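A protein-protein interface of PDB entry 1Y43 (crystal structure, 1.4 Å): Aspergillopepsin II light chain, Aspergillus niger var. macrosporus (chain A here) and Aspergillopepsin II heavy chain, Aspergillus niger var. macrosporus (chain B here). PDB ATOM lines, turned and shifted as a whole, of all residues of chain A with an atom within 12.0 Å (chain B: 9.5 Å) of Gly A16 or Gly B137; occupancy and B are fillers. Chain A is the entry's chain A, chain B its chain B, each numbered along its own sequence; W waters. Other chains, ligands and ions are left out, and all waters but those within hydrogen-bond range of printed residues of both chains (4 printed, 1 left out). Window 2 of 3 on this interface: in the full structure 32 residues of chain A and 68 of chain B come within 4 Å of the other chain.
N of Leu A12 sits at hydrogen-bond distance from O of Ala B105 (2.8 Å).
N of Gly A14 lies within hydrogen-bond range of O of Thr B103, 2.9 Å away.
The backbone carbonyl oxygen (O) of Asp A15 lies within hydrogen-bond range of the side-chain hydroxyl (OG) of Ser B136 (2.6 Å).
The backbone NH (N) of Gly A16 is in hydrogen-bond range of the backbone carbonyl oxygen (O) of Glu B102.
The backbone carbonyl oxygen (O) of Glu B102 is in hydrogen-bond range of the backbone NH (N) of Tyr A17, at 3.1 Å.
The backbone carbonyl oxygen (O) of Thr A18 lies within hydrogen-bond range of the backbone NH (N) of Ala B69.
The backbone NH (N) of Thr A18 sits at hydrogen-bond distance from the backbone carbonyl oxygen (O) of Thr B135, 2.9 Å away.
The backbone NH (N) of Thr B135 sits at hydrogen-bond distance from the backbone carbonyl oxygen (O) of Lys A19, 2.8 Å away.
The side-chain carboxylate of Asp B14 lies within hydrogen-bond range of the backbone NH of Glu B102.
N of Thr B103 lies within hydrogen-bond range of OD1 of Asp B14, at 2.9 Å.
The backbone NH (N) of Asp B14 sits at hydrogen-bond distance from the backbone carbonyl oxygen (O) of Asn B104 (2.8 Å).
O of Ala B134 sits at hydrogen-bond distance from N of Val B141, 2.8 Å away.
The backbone carbonyl oxygen (O) of Ser B136 sits at hydrogen-bond distance from the side-chain hydroxyl (OG) of Ser B139 (3.1 Å).
Among the printed residues, merely in contact across the chains: Leu A12 with Asn B104 (3.2 Å), Lys A19 with Ala B134 (3.3 Å), Tyr A17 with Thr B135 (3.3 Å), Ile A13 with Thr B103 (3.4 Å), Gly A16 with Ser B136 (3.4 Å), Tyr A17 with Thr B103 (3.5 Å), Leu A12 with Thr B103 (3.5 Å), Asp A15 with Glu B102 (3.5 Å), Val A20 with Ala B105 (3.6 Å), Val A20 with Ile B13 (3.7 Å), Gly A16 with Gly B137 (3.7 Å), Leu A12 with Val B141 (3.7 Å), Asp A15 with Thr B103 (3.7 Å), Tyr A17 with Ser B136 (3.7 Å), Gly A16 with Thr B135 (3.7 Å), Tyr A17 with Asn B104 (3.8 Å), Tyr A17 with Ala B105 (3.8 Å), Tyr A17 with Ile B13 (3.9 Å), Leu A12 with Ala B134 (3.9 Å), Thr A18 with Ile B13 (3.9 Å) and Thr A18 with Glu B102 (3.9 Å).
Of chain B, only Glu B102, Thr B135, Ser B136 and Gly B137 come within 4 Å of Gly A16.
Of chain A, only Gly A16 (3.7 Å) comes within 4 Å of Gly B137.
Glu B102 touches just these residues of chain A: Asp A15 (3.5 Å), Gly A16 (3.1 Å), Tyr A17 (3.1 Å) and Thr A18 (3.9 Å).
Of the printed residues of chain A, Thr B135 touches Gly A16 (3.7 Å), Tyr A17 (3.3 Å), Thr A18 (2.9 Å) and Lys A19 (2.8 Å).
No residue of chain A comes within 4 Å of Gly B138.
No residue of chain A comes within 4 Å of Ser B139.
Printed residues of chain A within 4 Å of Ala B105: Leu A12 (2.8 Å), Tyr A17 (3.8 Å) and Val A20 (3.6 Å).
Printed residues of chain B within 4 Å of Gly A14: Thr B103.
Of the printed residues of chain B, Tyr A17 touches Ile B13, Glu B102, Thr B103, Asn B104, Ala B105, Thr B135 and Ser B136.
The nearest residue of chain A that does not touch Gly B137 is Asp A15 (5.2 Å).
The nearest printed residue of chain A that does not touch Ile B13 is Lys A19 (4.1 Å).
Printed residues of chain A that touch a printed residue of chain B: Leu A12, Ile A13, Gly A14, Asp A15, Gly A16, Tyr A17, Thr A18, Lys A19 and Val A20.
Hydrophobic or aromatic side chains of chain A within 4 Å of the printed part of chain B: Leu A12, Tyr A17 and Val A20.
Among the printed residues, 29 pairs touch across the chains.
Among the printed residues, no Asp or Glu carboxylate lies within 4 Å of a Lys or Arg side-chain nitrogen of the other chain.
Water W1 bridges the side-chain hydroxyl of Ser B136 (2.9 Å) and the backbone carbonyl oxygen of Asp A15 (3.0 Å).
Water W2 bridges O of Gly A16 (2.9 Å) and N of Gly B137 (3.3 Å).
Water W3 bridges O of Asp A15 (2.9 Å) and OG of Ser B136 (3.3 Å).
Water W4 lies within hydrogen-bond range of the side-chain hydroxyl (OG1) of Thr A18, the backbone NH (N) of Gly B138 and the backbone NH (N) of Gly B137.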
ATOM      1  N   LEU A  12      10.656  -8.408 -11.277  1.00  0.00           N
ATOM      2  CA  LEU A  12       9.714  -7.409 -10.784  1.00  0.00           C
ATOM      3  C   LEU A  12       8.411  -8.144 -10.501  1.00  0.00           C
ATOM      4  O   LEU A  12       7.980  -8.978 -11.299  1.00  0.00           O
ATOM      5  CB  LEU A  12       9.439  -6.326 -11.831  1.00  0.00           C
ATOM      6  CG  LEU A  12      10.485  -5.232 -12.041  1.00  0.00           C
ATOM      7  CD1 LEU A  12      10.065  -4.397 -13.231  1.00  0.00           C
ATOM      8  CD2 LEU A  12      10.623  -4.361 -10.796  1.00  0.00           C
ATOM      9  N   ILE A  13       7.827  -7.884  -9.332  1.00  0.00           N
ATOM     10  CA  ILE A  13       6.550  -8.483  -8.971  1.00  0.00           C
ATOM     11  C   ILE A  13       5.530  -7.340  -8.858  1.00  0.00           C
ATOM     12  O   ILE A  13       5.731  -6.388  -8.099  1.00  0.00           O
ATOM     13  CB  ILE A  13       6.639  -9.254  -7.644  1.00  0.00           C
ATOM     14  CG1 ILE A  13       7.729 -10.332  -7.731  1.00  0.00           C
ATOM     15  CG2 ILE A  13       5.289  -9.915  -7.331  1.00  0.00           C
ATOM     16  CD1 ILE A  13       7.992 -11.051  -6.404  1.00  0.00           C
ATOM     17  N   GLY A  14       4.474  -7.415  -9.657  1.00  0.00           N
ATOM     18  CA  GLY A  14       3.457  -6.388  -9.643  1.00  0.00           C
ATOM     19  C   GLY A  14       2.270  -6.820 -10.475  1.00  0.00           C
ATOM     20  O   GLY A  14       1.855  -7.971 -10.420  1.00  0.00           O
ATOM     21  N   ASP A  15       1.753  -5.912 -11.296  1.00  0.00           N
ATOM     22  CA  ASP A  15       0.588  -6.206 -12.121  1.00  0.00           C
ATOM     23  C   ASP A  15       0.629  -5.465 -13.443  1.00  0.00           C
ATOM     24  O   ASP A  15       1.238  -4.399 -13.537  1.00  0.00           O
ATOM     25  CB  ASP A  15      -0.703  -5.791 -11.398  1.00  0.00           C
ATOM     26  CG  ASP A  15      -1.059  -6.714 -10.264  1.00  0.00           C
ATOM     27  OD1 ASP A  15      -1.556  -7.830 -10.556  1.00  0.00           O
ATOM     28  OD2 ASP A  15      -0.849  -6.315  -9.091  1.00  0.00           O
ATOM     29  N   GLY A  16      -0.010  -6.045 -14.450  1.00  0.00           N
ATOM     30  CA  GLY A  16      -0.118  -5.411 -15.755  1.00  0.00           C
ATOM     31  C   GLY A  16       1.080  -5.349 -16.686  1.00  0.00           C
ATOM     32  O   GLY A  16       1.059  -4.557 -17.631  1.00  0.00           O
ATOM     33  N   TYR A  17       2.102  -6.171 -16.462  1.00  0.00           N
ATOM     34  CA  TYR A  17       3.269  -6.148 -17.344  1.00  0.00           C
ATOM     35  C   TYR A  17       2.910  -6.670 -18.725  1.00  0.00           C
ATOM     36  O   TYR A  17       2.451  -7.810 -18.856  1.00  0.00           O
ATOM     37  CB  TYR A  17       4.413  -6.988 -16.760  1.00  0.00           C
ATOM     38  CG  TYR A  17       4.917  -6.476 -15.435  1.00  0.00           C
ATOM     39  CD1 TYR A  17       5.460  -5.192 -15.322  1.00  0.00           C
ATOM     40  CD2 TYR A  17       4.807  -7.251 -14.285  1.00  0.00           C
ATOM     41  CE1 TYR A  17       5.879  -4.693 -14.082  1.00  0.00           C
ATOM     42  CE2 TYR A  17       5.222  -6.766 -13.047  1.00  0.00           C
ATOM     43  CZ  TYR A  17       5.750  -5.491 -12.950  1.00  0.00           C
ATOM     44  OH  TYR A  17       6.129  -5.034 -11.711  1.00  0.00           O
ATOM     45  N   THR A  18       3.112  -5.843 -19.753  1.00  0.00           N
ATOM     46  CA  THR A  18       2.814  -6.261 -21.119  1.00  0.00           C
ATOM     47  C   THR A  18       4.025  -6.215 -22.061  1.00  0.00           C
ATOM     48  O   THR A  18       3.922  -6.599 -23.223  1.00  0.00           O
ATOM     49  CB  THR A  18       1.678  -5.422 -21.738  1.00  0.00           C
ATOM     50  OG1 THR A  18       2.080  -4.046 -21.790  1.00  0.00           O
ATOM     51  CG2 THR A  18       0.390  -5.560 -20.909  1.00  0.00           C
ATOM     52  N   LYS A  19       5.162  -5.736 -21.567  1.00  0.00           N
ATOM     53  CA  LYS A  19       6.373  -5.668 -22.385  1.00  0.00           C
ATOM     54  C   LYS A  19       7.600  -5.668 -21.490  1.00  0.00           C
ATOM     55  O   LYS A  19       7.591  -5.046 -20.423  1.00  0.00           O
ATOM     56  CB  LYS A  19       6.375  -4.398 -23.249  1.00  0.00           C
ATOM     57  CG  LYS A  19       7.630  -4.212 -24.091  1.00  0.00           C
ATOM     58  CD  LYS A  19       7.603  -2.907 -24.845  1.00  0.00           C
ATOM     59  CE  LYS A  19       9.014  -2.449 -25.133  1.00  0.00           C
ATOM     60  NZ  LYS A  19       9.019  -1.039 -25.591  1.00  0.00           N
ATOM     61  N   VAL A  20       8.612  -6.450 -21.870  1.00  0.00           N
ATOM     62  CA  VAL A  20       9.869  -6.489 -21.125  1.00  0.00           C
ATOM     63  C   VAL A  20      10.959  -6.524 -22.181  1.00  0.00           C
ATOM     64  O   VAL A  20      10.869  -7.283 -23.153  1.00  0.00           O
ATOM     65  CB  VAL A  20      10.017  -7.737 -20.228  1.00  0.00           C
ATOM     66  CG1 VAL A  20      11.302  -7.629 -19.414  1.00  0.00           C
ATOM     67  CG2 VAL A  20       8.815  -7.888 -19.318  1.00  0.00           C
ATOM     68  N   THR A  21      11.977  -5.695 -22.012  1.00  0.00           N
ATOM     69  CA  THR A  21      13.059  -5.649 -22.971  1.00  0.00           C
ATOM     70  C   THR A  21      14.402  -5.456 -22.269  1.00  0.00           C
ATOM     71  O   THR A  21      14.457  -4.997 -21.124  1.00  0.00           O
ATOM     72  CB  THR A  21      12.816  -4.533 -24.027  1.00  0.00           C
ATOM     73  OG1 THR A  21      13.839  -4.577 -25.022  1.00  0.00           O
ATOM     74  CG2 THR A  21      12.797  -3.141 -23.384  1.00  0.00           C
ATOM     75  N   ILE B  13       7.980 -12.637 -19.170  1.00  0.00           N
ATOM     76  CA  ILE B  13       6.831 -12.268 -18.361  1.00  0.00           C
ATOM     77  C   ILE B  13       6.346 -13.553 -17.668  1.00  0.00           C
ATOM     78  O   ILE B  13       6.198 -14.599 -18.312  1.00  0.00           O
ATOM     79  CB  ILE B  13       5.691 -11.700 -19.241  1.00  0.00           C
ATOM     80  CG1 ILE B  13       6.147 -10.375 -19.873  1.00  0.00           C
ATOM     81  CG2 ILE B  13       4.413 -11.499 -18.413  1.00  0.00           C
ATOM     82  CD1 ILE B  13       5.145  -9.762 -20.851  1.00  0.00           C
ATOM     83  N   ASP B  14       6.166 -13.457 -16.352  1.00  0.00           N
ATOM     84  CA  ASP B  14       5.673 -14.540 -15.508  1.00  0.00           C
ATOM     85  C   ASP B  14       6.620 -15.700 -15.261  1.00  0.00           C
ATOM     86  O   ASP B  14       7.787 -15.647 -15.655  1.00  0.00           O
ATOM     87  CB  ASP B  14       4.294 -15.002 -15.992  1.00  0.00           C
ATOM     88  CG  ASP B  14       3.242 -13.904 -15.849  1.00  0.00           C
ATOM     89  OD1 ASP B  14       3.358 -13.095 -14.910  1.00  0.00           O
ATOM     90  OD2 ASP B  14       2.315 -13.844 -16.677  1.00  0.00           O
ATOM     91  N   ALA B  69       3.013  -8.833 -24.641  1.00  0.00           N
ATOM     92  CA  ALA B  69       1.762  -9.572 -24.505  1.00  0.00           C
ATOM     93  C   ALA B  69       0.633  -8.674 -24.979  1.00  0.00           C
ATOM     94  O   ALA B  69       0.476  -7.569 -24.465  1.00  0.00           O
ATOM     95  CB  ALA B  69       1.528  -9.955 -23.050  1.00  0.00           C
ATOM     96  N   LYS B  72      -3.702 -12.019 -22.432  1.00  0.00           N
ATOM     97  CA  LYS B  72      -3.143 -13.062 -21.574  1.00  0.00           C
ATOM     98  C   LYS B  72      -2.802 -14.345 -22.335  1.00  0.00           C
ATOM     99  O   LYS B  72      -2.114 -15.215 -21.803  1.00  0.00           O
ATOM    100  CB  LYS B  72      -4.078 -13.363 -20.400  1.00  0.00           C
ATOM    101  CG  LYS B  72      -4.116 -12.246 -19.369  1.00  0.00           C
ATOM    102  CD  LYS B  72      -5.091 -12.588 -18.271  1.00  0.00           C
ATOM    103  CE  LYS B  72      -5.216 -11.476 -17.235  1.00  0.00           C
ATOM    104  NZ  LYS B  72      -6.527 -11.609 -16.506  1.00  0.00           N
ATOM    105  N   LEU B 100      -1.178 -16.012 -19.241  1.00  0.00           N
ATOM    106  CA  LEU B 100      -0.287 -15.193 -18.442  1.00  0.00           C
ATOM    107  C   LEU B 100      -1.083 -14.533 -17.319  1.00  0.00           C
ATOM    108  O   LEU B 100      -2.295 -14.369 -17.430  1.00  0.00           O
ATOM    109  CB  LEU B 100       0.289 -14.072 -19.298  1.00  0.00           C
ATOM    110  CG  LEU B 100       1.202 -14.474 -20.443  1.00  0.00           C
ATOM    111  CD1 LEU B 100       1.548 -13.228 -21.259  1.00  0.00           C
ATOM    112  CD2 LEU B 100       2.449 -15.132 -19.868  1.00  0.00           C
ATOM    113  N   CYS B 101      -0.412 -14.205 -16.219  1.00  0.00           N
ATOM    114  CA  CYS B 101      -1.044 -13.466 -15.121  1.00  0.00           C
ATOM    115  C   CYS B 101      -0.601 -12.008 -15.270  1.00  0.00           C
ATOM    116  O   CYS B 101      -1.253 -11.099 -14.769  1.00  0.00           O
ATOM    117  CB  CYS B 101      -0.541 -13.917 -13.752  1.00  0.00           C
ATOM    118  SG  CYS B 101      -0.608 -15.678 -13.389  1.00  0.00           S
ATOM    119  N   GLU B 102       0.559 -11.818 -15.907  1.00  0.00           N
ATOM    120  CA  GLU B 102       1.179 -10.509 -16.111  1.00  0.00           C
ATOM    121  C   GLU B 102       1.627  -9.887 -14.786  1.00  0.00           C
ATOM    122  O   GLU B 102       1.609  -8.666 -14.608  1.00  0.00           O
ATOM    123  CB  GLU B 102       0.265  -9.582 -16.926  1.00  0.00           C
ATOM    124  CG  GLU B 102       0.000 -10.122 -18.319  1.00  0.00           C
ATOM    125  CD  GLU B 102      -0.839  -9.208 -19.195  1.00  0.00           C
ATOM    126  OE1 GLU B 102      -1.425  -8.226 -18.695  1.00  0.00           O
ATOM    127  OE2 GLU B 102      -0.894  -9.488 -20.406  1.00  0.00           O
ATOM    128  N   THR B 103       2.085 -10.748 -13.874  1.00  0.00           N
ATOM    129  CA  THR B 103       2.536 -10.312 -12.559  1.00  0.00           C
ATOM    130  C   THR B 103       4.046 -10.301 -12.369  1.00  0.00           C
ATOM    131  O   THR B 103       4.529  -9.780 -11.371  1.00  0.00           O
ATOM    132  CB  THR B 103       1.867 -11.127 -11.421  1.00  0.00           C
ATOM    133  OG1 THR B 103       2.126 -12.517 -11.615  1.00  0.00           O
ATOM    134  CG2 THR B 103       0.350 -10.888 -11.414  1.00  0.00           C
ATOM    135  N   ASN B 104       4.797 -10.909 -13.287  1.00  0.00           N
ATOM    136  CA  ASN B 104       6.265 -10.886 -13.170  1.00  0.00           C
ATOM    137  C   ASN B 104       6.903 -10.425 -14.488  1.00  0.00           C
ATOM    138  O   ASN B 104       6.409 -10.760 -15.567  1.00  0.00           O
ATOM    139  CB  ASN B 104       6.847 -12.272 -12.904  1.00  0.00           C
ATOM    140  CG  ASN B 104       6.156 -13.028 -11.801  1.00  0.00           C
ATOM    141  OD1 ASN B 104       6.072 -14.249 -11.851  1.00  0.00           O
ATOM    142  ND2 ASN B 104       5.705 -12.312 -10.770  1.00  0.00           N
ATOM    143  N   ALA B 105       7.955  -9.620 -14.386  1.00  0.00           N
ATOM    144  CA  ALA B 105       8.730  -9.151 -15.542  1.00  0.00           C
ATOM    145  C   ALA B 105      10.148  -9.453 -15.072  1.00  0.00           C
ATOM    146  O   ALA B 105      10.516  -9.081 -13.960  1.00  0.00           O
ATOM    147  CB  ALA B 105       8.551  -7.642 -15.763  1.00  0.00           C
ATOM    148  N   ALA B 134      10.544  -2.521 -18.254  1.00  0.00           N
ATOM    149  CA  ALA B 134       9.286  -3.270 -18.292  1.00  0.00           C
ATOM    150  C   ALA B 134       8.166  -2.235 -18.412  1.00  0.00           C
ATOM    151  O   ALA B 134       8.283  -1.136 -17.869  1.00  0.00           O
ATOM    152  CB  ALA B 134       9.111  -4.089 -17.009  1.00  0.00           C
ATOM    153  N   THR B 135       7.093  -2.570 -19.117  1.00  0.00           N
ATOM    154  CA  THR B 135       5.977  -1.649 -19.282  1.00  0.00           C
ATOM    155  C   THR B 135       4.765  -2.226 -18.577  1.00  0.00           C
ATOM    156  O   THR B 135       4.389  -3.370 -18.815  1.00  0.00           O
ATOM    157  CB  THR B 135       5.668  -1.414 -20.763  1.00  0.00           C
ATOM    158  OG1 THR B 135       6.857  -0.952 -21.410  1.00  0.00           O
ATOM    159  CG2 THR B 135       4.578  -0.361 -20.933  1.00  0.00           C
ATOM    160  N   SER B 136       4.168  -1.415 -17.713  1.00  0.00           N
ATOM    161  CA  SER B 136       3.004  -1.800 -16.932  1.00  0.00           C
ATOM    162  C   SER B 136       2.029  -0.632 -16.957  1.00  0.00           C
ATOM    163  O   SER B 136       2.402   0.490 -16.641  1.00  0.00           O
ATOM    164  CB  SER B 136       3.430  -2.087 -15.486  1.00  0.00           C
ATOM    165  OG  SER B 136       2.305  -2.334 -14.664  1.00  0.00           O
ATOM    166  N   GLY B 137       0.787  -0.887 -17.362  1.00  0.00           N
ATOM    167  CA  GLY B 137      -0.205   0.175 -17.408  1.00  0.00           C
ATOM    168  C   GLY B 137       0.183   1.357 -18.279  1.00  0.00           C
ATOM    169  O   GLY B 137      -0.252   2.490 -18.036  1.00  0.00           O
ATOM    170  N   GLY B 138       1.008   1.094 -19.289  1.00  0.00           N
ATOM    171  CA  GLY B 138       1.443   2.140 -20.202  1.00  0.00           C
ATOM    172  C   GLY B 138       2.689   2.896 -19.773  1.00  0.00           C
ATOM    173  O   GLY B 138       3.241   3.670 -20.572  1.00  0.00           O
ATOM    174  N   SER B 139       3.141   2.664 -18.536  1.00  0.00           N
ATOM    175  CA  SER B 139       4.319   3.329 -17.966  1.00  0.00           C
ATOM    176  C   SER B 139       5.528   2.386 -17.895  1.00  0.00           C
ATOM    177  O   SER B 139       5.372   1.195 -17.645  1.00  0.00           O
ATOM    178  CB  SER B 139       3.988   3.867 -16.562  1.00  0.00           C
ATOM    179  OG  SER B 139       4.110   2.870 -15.543  1.00  0.00           O
ATOM    180  N   THR B 140       6.727   2.917 -18.124  1.00  0.00           N
ATOM    181  CA  THR B 140       7.938   2.099 -18.079  1.00  0.00           C
ATOM    182  C   THR B 140       8.642   2.184 -16.726  1.00  0.00           C
ATOM    183  O   THR B 140       8.735   3.261 -16.117  1.00  0.00           O
ATOM    184  CB  THR B 140       8.929   2.472 -19.206  1.00  0.00           C
ATOM    185  OG1 THR B 140       9.372   3.819 -19.021  1.00  0.00           O
ATOM    186  CG2 THR B 140       8.262   2.352 -20.564  1.00  0.00           C
ATOM    187  N   VAL B 141       9.131   1.042 -16.252  1.00  0.00           N
ATOM    188  CA  VAL B 141       9.843   0.964 -14.976  1.00  0.00           C
ATOM    189  C   VAL B 141      11.091   0.133 -15.167  1.00  0.00           C
ATOM    190  O   VAL B 141      11.140  -0.760 -16.025  1.00  0.00           O
ATOM    191  CB  VAL B 141       8.996   0.288 -13.855  1.00  0.00           C
ATOM    192  CG1 VAL B 141       7.716   1.092 -13.572  1.00  0.00           C
ATOM    193  CG2 VAL B 141       8.644  -1.143 -14.235  1.00  0.00           C
HETATM  194  O   HOH W   1      -0.105  -1.688 -13.249  1.00  0.00           O
HETATM  195  O   HOH W   2      -1.301  -3.101 -18.578  1.00  0.00           O
HETATM  196  O   HOH W   3       2.804  -3.047 -11.457  1.00  0.00           O
HETATM  197  O   HOH W   4       1.020  -1.692 -20.374  1.00  0.00           O
